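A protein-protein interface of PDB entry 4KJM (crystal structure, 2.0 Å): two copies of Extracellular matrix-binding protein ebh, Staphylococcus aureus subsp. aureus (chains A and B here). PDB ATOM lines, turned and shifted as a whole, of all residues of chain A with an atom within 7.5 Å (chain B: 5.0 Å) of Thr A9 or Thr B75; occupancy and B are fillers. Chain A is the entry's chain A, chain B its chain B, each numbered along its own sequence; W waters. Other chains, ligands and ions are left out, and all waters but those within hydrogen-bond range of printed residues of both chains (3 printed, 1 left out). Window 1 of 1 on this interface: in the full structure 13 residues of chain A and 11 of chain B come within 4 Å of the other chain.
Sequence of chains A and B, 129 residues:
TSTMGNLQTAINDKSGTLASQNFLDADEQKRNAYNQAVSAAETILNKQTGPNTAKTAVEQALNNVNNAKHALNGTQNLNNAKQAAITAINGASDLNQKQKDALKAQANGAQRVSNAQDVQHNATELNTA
The side-chain amino group (NZ) of Lys B82 lies within hydrogen-bond range of the side-chain hydroxyl (OG1) of Thr A9, at 2.8 Å. NZ of Lys B82 lies within hydrogen-bond range of O of Gly A5 (3.1 Å). The side-chain amide oxygen (OD1) of Asn B79 is in hydrogen-bond range of the side-chain hydroxyl (OG1) of Thr A9 (2.6 Å).
O of Gly A5 is in hydrogen-bond range of OG1 of Thr A9, 3.0 Å away. OD1 of Asn B22 is in hydrogen-bond range of N of Thr B75. The backbone carbonyl oxygen (O) of Ser A2 lies close to the side-chain amide oxygen (OD1) of Asn A6.
Gly A5 touches Asn B79 (O to OD1, 3.8 Å). OD1 of Asn A6 touches OD1 of Asn B79 (3.5 Å). Gln A8 touches Lys B82 (CB to NZ, 3.8 Å). Thr B75 touches Thr A9 (CG2 to CG2, 3.6 Å).
Printed residues of chain B within 4 Å of Gly A5: Asn B79 and Lys B82. Printed residues of chain B within 4 Å of Asn A6: Asn B79. Printed residues of chain B within 4 Å of Gln A8: Lys B82 (3.8 Å). Thr A9 touches just these residues of chain B: Thr B75 (3.6 Å), Asn B79 (2.6 Å) and Lys B82 (2.8 Å). Asn A66 touches none of the printed residues of chain B. Of chain A, only Thr A9 comes within 4 Å of Thr B75. Asn B77 touches none of the printed residues of chain A. Printed residues of chain A within 4 Å of Asn B79: Gly A5, Asn A6 and Thr A9. Of the printed residues of chain A, Lys B82 touches Gly A5 (3.1 Å), Gln A8 (3.8 Å) and Thr A9 (2.8 Å). The nearest residue of chain B that does not touch Thr A9 is Leu B78 (4.1 Å). The nearest residue of chain A that does not touch Thr B75 is Asp A13 (6.0 Å). The nearest printed residue of chain B that does not touch Asn A6 is Gln B76 (4.7 Å).
Of the 10 printed residues of chain B, 3 touch a printed residue of chain A. Among the printed residues, no Asp or Glu carboxylate lies within 4 Å of a Lys or Arg side-chain nitrogen of the other chain.
No position is printed for both chains. Of the 7 pairs that touch across the chains among the printed residues, none has its exchanged pair printed and touching as well.
Water W1 bridges OD1 of Asn A6 (2.7 Å) and O of Asn B79 (3.4 Å). Water W2 bridges NZ of Lys B82 (2.8 Å) and ND2 of Asn A12 (2.8 Å). Water W3 lies within hydrogen-bond range of O of Asn A6 (2.8 Å) and ND2 of Asn B79 (3.1 Å).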
ATOM      1  N   SER A   2       3.493  34.941  -5.076  1.00  0.00           N
ATOM      2  CA  SER A   2       2.939  33.614  -5.231  1.00  0.00           C
ATOM      3  C   SER A   2       3.867  32.649  -4.498  1.00  0.00           C
ATOM      4  O   SER A   2       3.410  31.678  -3.899  1.00  0.00           O
ATOM      5  CB  SER A   2       2.766  33.242  -6.706  1.00  0.00           C
ATOM      6  OG  SER A   2       3.921  32.624  -7.198  1.00  0.00           O
ATOM      7  N   THR A   3       5.169  32.949  -4.533  1.00  0.00           N
ATOM      8  CA  THR A   3       6.106  32.209  -3.763  1.00  0.00           C
ATOM      9  C   THR A   3       5.762  32.468  -2.262  1.00  0.00           C
ATOM     10  O   THR A   3       5.685  31.510  -1.558  1.00  0.00           O
ATOM     11  CB  THR A   3       7.615  32.440  -4.118  1.00  0.00           C
ATOM     12  OG1 THR A   3       7.818  32.347  -5.521  1.00  0.00           O
ATOM     13  CG2 THR A   3       8.499  31.351  -3.478  1.00  0.00           C
ATOM     14  N   MET A   4       5.476  33.686  -1.799  1.00  0.00           N
ATOM     15  CA  MET A   4       5.184  33.870  -0.343  1.00  0.00           C
ATOM     16  C   MET A   4       3.989  33.009   0.087  1.00  0.00           C
ATOM     17  O   MET A   4       4.050  32.335   1.100  1.00  0.00           O
ATOM     18  CB  MET A   4       5.018  35.303   0.134  1.00  0.00           C
ATOM     19  CG  MET A   4       6.341  36.054   0.172  1.00  0.00           C
ATOM     20  SD  MET A   4       7.484  35.600   1.722  1.00  0.00           S
ATOM     21  CE  MET A   4       8.624  37.204   1.790  1.00  0.00           C
ATOM     22  N   GLY A   5       2.904  33.044  -0.666  1.00  0.00           N
ATOM     23  CA  GLY A   5       1.752  32.202  -0.456  1.00  0.00           C
ATOM     24  C   GLY A   5       2.049  30.703  -0.379  1.00  0.00           C
ATOM     25  O   GLY A   5       1.536  29.999   0.474  1.00  0.00           O
ATOM     26  N   ASN A   6       2.845  30.220  -1.310  1.00  0.00           N
ATOM     27  CA  ASN A   6       3.272  28.829  -1.300  1.00  0.00           C
ATOM     28  C   ASN A   6       4.082  28.506  -0.053  1.00  0.00           C
ATOM     29  O   ASN A   6       3.949  27.432   0.485  1.00  0.00           O
ATOM     30  CB  ASN A   6       4.062  28.486  -2.545  1.00  0.00           C
ATOM     31  CG  ASN A   6       3.174  28.162  -3.720  1.00  0.00           C
ATOM     32  OD1 ASN A   6       2.232  28.869  -4.002  1.00  0.00           O
ATOM     33  ND2 ASN A   6       3.463  27.062  -4.398  1.00  0.00           N
ATOM     34  N   LEU A   7       4.963  29.410   0.361  1.00  0.00           N
ATOM     35  CA  LEU A   7       5.782  29.177   1.534  1.00  0.00           C
ATOM     36  C   LEU A   7       4.903  29.054   2.767  1.00  0.00           C
ATOM     37  O   LEU A   7       5.062  28.178   3.585  1.00  0.00           O
ATOM     38  CB  LEU A   7       6.792  30.335   1.702  1.00  0.00           C
ATOM     39  CG  LEU A   7       7.848  30.165   2.819  1.00  0.00           C
ATOM     40  CD1 LEU A   7       8.617  28.879   2.657  1.00  0.00           C
ATOM     41  CD2 LEU A   7       8.775  31.344   2.866  1.00  0.00           C
ATOM     42  N   GLN A   8       3.930  29.950   2.867  1.00  0.00           N
ATOM     43  CA  GLN A   8       2.951  29.940   3.955  1.00  0.00           C
ATOM     44  C   GLN A   8       2.201  28.645   4.009  1.00  0.00           C
ATOM     45  O   GLN A   8       1.971  28.121   5.082  1.00  0.00           O
ATOM     46  CB  GLN A   8       2.001  31.136   3.754  1.00  0.00           C
ATOM     47  CG  GLN A   8       2.700  32.427   4.060  1.00  0.00           C
ATOM     48  CD  GLN A   8       2.150  32.997   5.318  1.00  0.00           C
ATOM     49  OE1 GLN A   8       1.579  34.134   5.312  1.00  0.00           O
ATOM     50  NE2 GLN A   8       2.174  32.179   6.377  1.00  0.00           N
ATOM     51  N   THR A   9       1.786  28.144   2.834  1.00  0.00           N
ATOM     52  CA  THR A   9       1.104  26.854   2.744  1.00  0.00           C
ATOM     53  C   THR A   9       1.989  25.725   3.455  1.00  0.00           C
ATOM     54  O   THR A   9       1.538  24.992   4.378  1.00  0.00           O
ATOM     55  CB  THR A   9       0.694  26.579   1.269  1.00  0.00           C
ATOM     56  OG1 THR A   9      -0.254  27.571   0.816  1.00  0.00           O
ATOM     57  CG2 THR A   9       0.072  25.237   1.117  1.00  0.00           C
ATOM     58  N   ALA A  10       3.294  25.713   3.163  1.00  0.00           N
ATOM     59  CA  ALA A  10       4.207  24.841   3.949  1.00  0.00           C
ATOM     60  C   ALA A  10       4.378  25.172   5.468  1.00  0.00           C
ATOM     61  O   ALA A  10       4.364  24.260   6.309  1.00  0.00           O
ATOM     62  CB  ALA A  10       5.527  24.785   3.193  1.00  0.00           C
ATOM     63  N   ILE A  11       4.556  26.403   5.917  1.00  0.00           N
ATOM     64  CA  ILE A  11       4.830  26.588   7.343  1.00  0.00           C
ATOM     65  C   ILE A  11       3.554  26.276   8.203  1.00  0.00           C
ATOM     66  O   ILE A  11       3.635  25.786   9.308  1.00  0.00           O
ATOM     67  CB  ILE A  11       5.567  27.906   7.757  1.00  0.00           C
ATOM     68  CG1 ILE A  11       4.645  29.007   8.098  1.00  0.00           C
ATOM     69  CG2 ILE A  11       6.544  28.404   6.726  1.00  0.00           C
ATOM     70  CD1 ILE A  11       4.461  29.186   9.581  1.00  0.00           C
ATOM     71  N   ASN A  12       2.390  26.580   7.666  1.00  0.00           N
ATOM     72  CA  ASN A  12       1.128  26.447   8.384  1.00  0.00           C
ATOM     73  C   ASN A  12       0.741  24.965   8.547  1.00  0.00           C
ATOM     74  O   ASN A  12      -0.195  24.617   9.237  1.00  0.00           O
ATOM     75  CB  ASN A  12       0.026  27.189   7.636  1.00  0.00           C
ATOM     76  CG  ASN A  12       0.059  28.691   7.833  1.00  0.00           C
ATOM     77  OD1 ASN A  12       0.728  29.202   8.724  1.00  0.00           O
ATOM     78  ND2 ASN A  12      -0.678  29.400   7.005  1.00  0.00           N
ATOM     79  N   ASP A  13       1.493  24.098   7.901  1.00  0.00           N
ATOM     80  CA  ASP A  13       1.257  22.677   8.045  1.00  0.00           C
ATOM     81  C   ASP A  13       2.130  21.972   9.082  1.00  0.00           C
ATOM     82  O   ASP A  13       2.025  20.800   9.318  1.00  0.00           O
ATOM     83  CB  ASP A  13       1.432  21.987   6.732  1.00  0.00           C
ATOM     84  CG  ASP A  13       0.879  20.628   6.751  1.00  0.00           C
ATOM     85  OD1 ASP A  13      -0.160  20.495   7.377  1.00  0.00           O
ATOM     86  OD2 ASP A  13       1.478  19.744   6.171  1.00  0.00           O
ATOM     87  N   LYS A  14       2.992  22.769   9.653  1.00  0.00           N
ATOM     88  CA  LYS A  14       3.928  22.430  10.663  1.00  0.00           C
ATOM     89  C   LYS A  14       3.303  21.567  11.760  1.00  0.00           C
ATOM     90  O   LYS A  14       3.748  20.492  12.029  1.00  0.00           O
ATOM     91  CB  LYS A  14       4.461  23.735  11.213  1.00  0.00           C
ATOM     92  CG  LYS A  14       5.413  23.678  12.372  1.00  0.00           C
ATOM     93  CD  LYS A  14       5.547  25.079  12.943  1.00  0.00           C
ATOM     94  CE  LYS A  14       6.126  25.167  14.339  1.00  0.00           C
ATOM     95  NZ  LYS A  14       6.964  26.396  14.519  1.00  0.00           N
ATOM     96  N   LEU A  45       8.881  34.578   6.608  1.00  0.00           N
ATOM     97  CA  LEU A  45       7.487  34.995   6.715  1.00  0.00           C
ATOM     98  C   LEU A  45       7.317  36.054   7.803  1.00  0.00           C
ATOM     99  O   LEU A  45       6.231  36.604   7.942  1.00  0.00           O
ATOM    100  CB  LEU A  45       6.583  33.803   6.996  1.00  0.00           C
ATOM    101  CG  LEU A  45       6.661  32.729   5.915  1.00  0.00           C
ATOM    102  CD1 LEU A  45       5.947  31.454   6.342  1.00  0.00           C
ATOM    103  CD2 LEU A  45       6.107  33.254   4.614  1.00  0.00           C
ATOM    104  N   LEU A  62      11.388  27.515   0.581  1.00  0.00           N
ATOM    105  CA  LEU A  62      10.290  26.630   0.215  1.00  0.00           C
ATOM    106  C   LEU A  62      10.783  25.241  -0.170  1.00  0.00           C
ATOM    107  O   LEU A  62      10.260  24.239   0.334  1.00  0.00           O
ATOM    108  CB  LEU A  62       9.496  27.237  -0.912  1.00  0.00           C
ATOM    109  CG  LEU A  62       8.375  26.463  -1.551  1.00  0.00           C
ATOM    110  CD1 LEU A  62       7.397  25.935  -0.551  1.00  0.00           C
ATOM    111  CD2 LEU A  62       7.677  27.411  -2.532  1.00  0.00           C
ATOM    112  N   VAL A  65      11.991  23.326   2.921  1.00  0.00           N
ATOM    113  CA  VAL A  65      10.894  22.717   3.645  1.00  0.00           C
ATOM    114  C   VAL A  65      10.333  21.501   2.895  1.00  0.00           C
ATOM    115  O   VAL A  65      10.120  20.470   3.514  1.00  0.00           O
ATOM    116  CB  VAL A  65       9.671  23.675   3.876  1.00  0.00           C
ATOM    117  CG1 VAL A  65       8.548  22.942   4.631  1.00  0.00           C
ATOM    118  CG2 VAL A  65      10.094  24.867   4.725  1.00  0.00           C
ATOM    119  N   ASN A  66      10.064  21.618   1.592  1.00  0.00           N
ATOM    120  CA  ASN A  66       9.459  20.507   0.883  1.00  0.00           C
ATOM    121  C   ASN A  66      10.375  19.271   0.889  1.00  0.00           C
ATOM    122  O   ASN A  66       9.933  18.171   1.124  1.00  0.00           O
ATOM    123  CB  ASN A  66       9.072  20.915  -0.544  1.00  0.00           C
ATOM    124  CG  ASN A  66       7.881  21.910  -0.566  1.00  0.00           C
ATOM    125  OD1 ASN A  66       7.137  21.995   0.346  1.00  0.00           O
ATOM    126  ND2 ASN A  66       7.760  22.645  -1.595  1.00  0.00           N
ATOM    127  N   LYS A  69      10.507  17.769   4.393  1.00  0.00           N
ATOM    128  CA  LYS A  69       9.283  17.077   4.674  1.00  0.00           C
ATOM    129  C   LYS A  69       9.206  15.710   3.932  1.00  0.00           C
ATOM    130  O   LYS A  69       8.815  14.690   4.502  1.00  0.00           O
ATOM    131  CB  LYS A  69       8.067  17.948   4.356  1.00  0.00           C
ATOM    132  CG  LYS A  69       6.787  17.306   4.869  1.00  0.00           C
ATOM    133  CD  LYS A  69       5.572  18.122   4.467  1.00  0.00           C
ATOM    134  CE  LYS A  69       4.313  17.507   5.045  1.00  0.00           C
ATOM    135  NZ  LYS A  69       3.203  18.488   4.858  1.00  0.00           N
ATOM    136  N   GLN B  21      -5.489  19.006   6.028  1.00  0.00           N
ATOM    137  CA  GLN B  21      -5.981  19.916   5.053  1.00  0.00           C
ATOM    138  C   GLN B  21      -5.824  19.323   3.650  1.00  0.00           C
ATOM    139  O   GLN B  21      -6.664  19.591   2.760  1.00  0.00           O
ATOM    140  CB  GLN B  21      -5.193  21.208   5.171  1.00  0.00           C
ATOM    141  CG  GLN B  21      -5.613  22.329   4.248  1.00  0.00           C
ATOM    142  CD  GLN B  21      -5.106  22.191   2.825  1.00  0.00           C
ATOM    143  OE1 GLN B  21      -3.996  21.706   2.584  1.00  0.00           O
ATOM    144  NE2 GLN B  21      -5.848  22.721   1.901  1.00  0.00           N
ATOM    145  N   ASN B  22      -4.787  18.521   3.408  1.00  0.00           N
ATOM    146  CA  ASN B  22      -4.539  17.968   2.087  1.00  0.00           C
ATOM    147  C   ASN B  22      -5.680  17.004   1.647  1.00  0.00           C
ATOM    148  O   ASN B  22      -6.019  16.920   0.491  1.00  0.00           O
ATOM    149  CB  ASN B  22      -3.202  17.263   2.065  1.00  0.00           C
ATOM    150  CG  ASN B  22      -2.808  16.784   0.639  1.00  0.00           C
ATOM    151  OD1 ASN B  22      -2.810  17.562  -0.317  1.00  0.00           O
ATOM    152  ND2 ASN B  22      -2.421  15.519   0.535  1.00  0.00           N
ATOM    153  N   ASN B  73      -5.249  16.228  -3.202  1.00  0.00           N
ATOM    154  CA  ASN B  73      -4.681  17.452  -3.717  1.00  0.00           C
ATOM    155  C   ASN B  73      -5.168  18.729  -3.037  1.00  0.00           C
ATOM    156  O   ASN B  73      -5.185  19.770  -3.648  1.00  0.00           O
ATOM    157  CB  ASN B  73      -4.945  17.527  -5.211  1.00  0.00           C
ATOM    158  CG  ASN B  73      -6.380  17.657  -5.518  1.00  0.00           C
ATOM    159  OD1 ASN B  73      -7.266  17.338  -4.728  1.00  0.00           O
ATOM    160  ND2 ASN B  73      -6.634  18.071  -6.701  1.00  0.00           N
ATOM    161  N   GLY B  74      -5.542  18.633  -1.757  1.00  0.00           N
ATOM    162  CA  GLY B  74      -5.907  19.804  -0.976  1.00  0.00           C
ATOM    163  C   GLY B  74      -4.877  20.907  -0.925  1.00  0.00           C
ATOM    164  O   GLY B  74      -5.244  22.103  -0.962  1.00  0.00           O
ATOM    165  N   THR B  75      -3.618  20.551  -0.774  1.00  0.00           N
ATOM    166  CA  THR B  75      -2.581  21.532  -0.655  1.00  0.00           C
ATOM    167  C   THR B  75      -2.492  22.329  -1.970  1.00  0.00           C
ATOM    168  O   THR B  75      -2.434  23.549  -1.966  1.00  0.00           O
ATOM    169  CB  THR B  75      -1.223  20.866  -0.367  1.00  0.00           C
ATOM    170  OG1 THR B  75      -1.325  20.138   0.844  1.00  0.00           O
ATOM    171  CG2 THR B  75      -0.166  21.871  -0.180  1.00  0.00           C
ATOM    172  N   GLN B  76      -2.426  21.600  -3.082  1.00  0.00           N
ATOM    173  CA  GLN B  76      -2.438  22.288  -4.400  1.00  0.00           C
ATOM    174  C   GLN B  76      -3.732  23.106  -4.616  1.00  0.00           C
ATOM    175  O   GLN B  76      -3.661  24.236  -5.070  1.00  0.00           O
ATOM    176  CB  GLN B  76      -2.117  21.333  -5.553  1.00  0.00           C
ATOM    177  CG  GLN B  76      -0.676  21.429  -6.026  1.00  0.00           C
ATOM    178  CD  GLN B  76      -0.075  22.871  -6.069  1.00  0.00           C
ATOM    179  OE1 GLN B  76       0.922  23.193  -5.356  1.00  0.00           O
ATOM    180  NE2 GLN B  76      -0.730  23.766  -6.837  1.00  0.00           N
ATOM    181  N   ASN B  77      -4.903  22.627  -4.139  1.00  0.00           N
ATOM    182  CA  ASN B  77      -6.130  23.413  -4.276  1.00  0.00           C
ATOM    183  C   ASN B  77      -6.055  24.743  -3.477  1.00  0.00           C
ATOM    184  O   ASN B  77      -6.573  25.795  -3.853  1.00  0.00           O
ATOM    185  CB  ASN B  77      -7.352  22.602  -3.865  1.00  0.00           C
ATOM    186  CG  ASN B  77      -7.793  21.630  -4.927  1.00  0.00           C
ATOM    187  OD1 ASN B  77      -7.342  21.734  -6.062  1.00  0.00           O
ATOM    188  ND2 ASN B  77      -8.599  20.625  -4.545  1.00  0.00           N
ATOM    189  N   LEU B  78      -5.460  24.656  -2.307  1.00  0.00           N
ATOM    190  CA  LEU B  78      -5.208  25.836  -1.514  1.00  0.00           C
ATOM    191  C   LEU B  78      -4.297  26.803  -2.175  1.00  0.00           C
ATOM    192  O   LEU B  78      -4.626  27.985  -2.247  1.00  0.00           O
ATOM    193  CB  LEU B  78      -4.702  25.429  -0.136  1.00  0.00           C
ATOM    194  CG  LEU B  78      -4.352  26.567   0.801  1.00  0.00           C
ATOM    195  CD1 LEU B  78      -5.495  27.562   1.013  1.00  0.00           C
ATOM    196  CD2 LEU B  78      -3.829  25.971   2.134  1.00  0.00           C
ATOM    197  N   ASN B  79      -3.141  26.347  -2.656  1.00  0.00           N
ATOM    198  CA  ASN B  79      -2.259  27.286  -3.404  1.00  0.00           C
ATOM    199  C   ASN B  79      -2.903  27.893  -4.626  1.00  0.00           C
ATOM    200  O   ASN B  79      -2.760  29.079  -4.862  1.00  0.00           O
ATOM    201  CB  ASN B  79      -0.938  26.622  -3.800  1.00  0.00           C
ATOM    202  CG  ASN B  79       0.003  26.482  -2.642  1.00  0.00           C
ATOM    203  OD1 ASN B  79       0.023  27.326  -1.732  1.00  0.00           O
ATOM    204  ND2 ASN B  79       0.768  25.359  -2.605  1.00  0.00           N
ATOM    205  N   LYS B  82      -5.349  30.560  -3.332  1.00  0.00           N
ATOM    206  CA  LYS B  82      -4.555  31.744  -2.972  1.00  0.00           C
ATOM    207  C   LYS B  82      -4.183  32.607  -4.200  1.00  0.00           C
ATOM    208  O   LYS B  82      -4.371  33.805  -4.191  1.00  0.00           O
ATOM    209  CB  LYS B  82      -3.309  31.353  -2.209  1.00  0.00           C
ATOM    210  CG  LYS B  82      -3.568  30.783  -0.836  1.00  0.00           C
ATOM    211  CD  LYS B  82      -2.247  30.505  -0.145  1.00  0.00           C
ATOM    212  CE  LYS B  82      -2.439  29.985   1.279  1.00  0.00           C
ATOM    213  NZ  LYS B  82      -1.123  29.953   2.020  1.00  0.00           N
HETATM  214  O   HOH W   1       0.098  30.415  -3.500  1.00  0.00           O
HETATM  215  O   HOH W   2      -1.506  28.594   4.422  1.00  0.00           O
HETATM  216  O   HOH W   3       3.113  24.982  -0.634  1.00  0.00           O
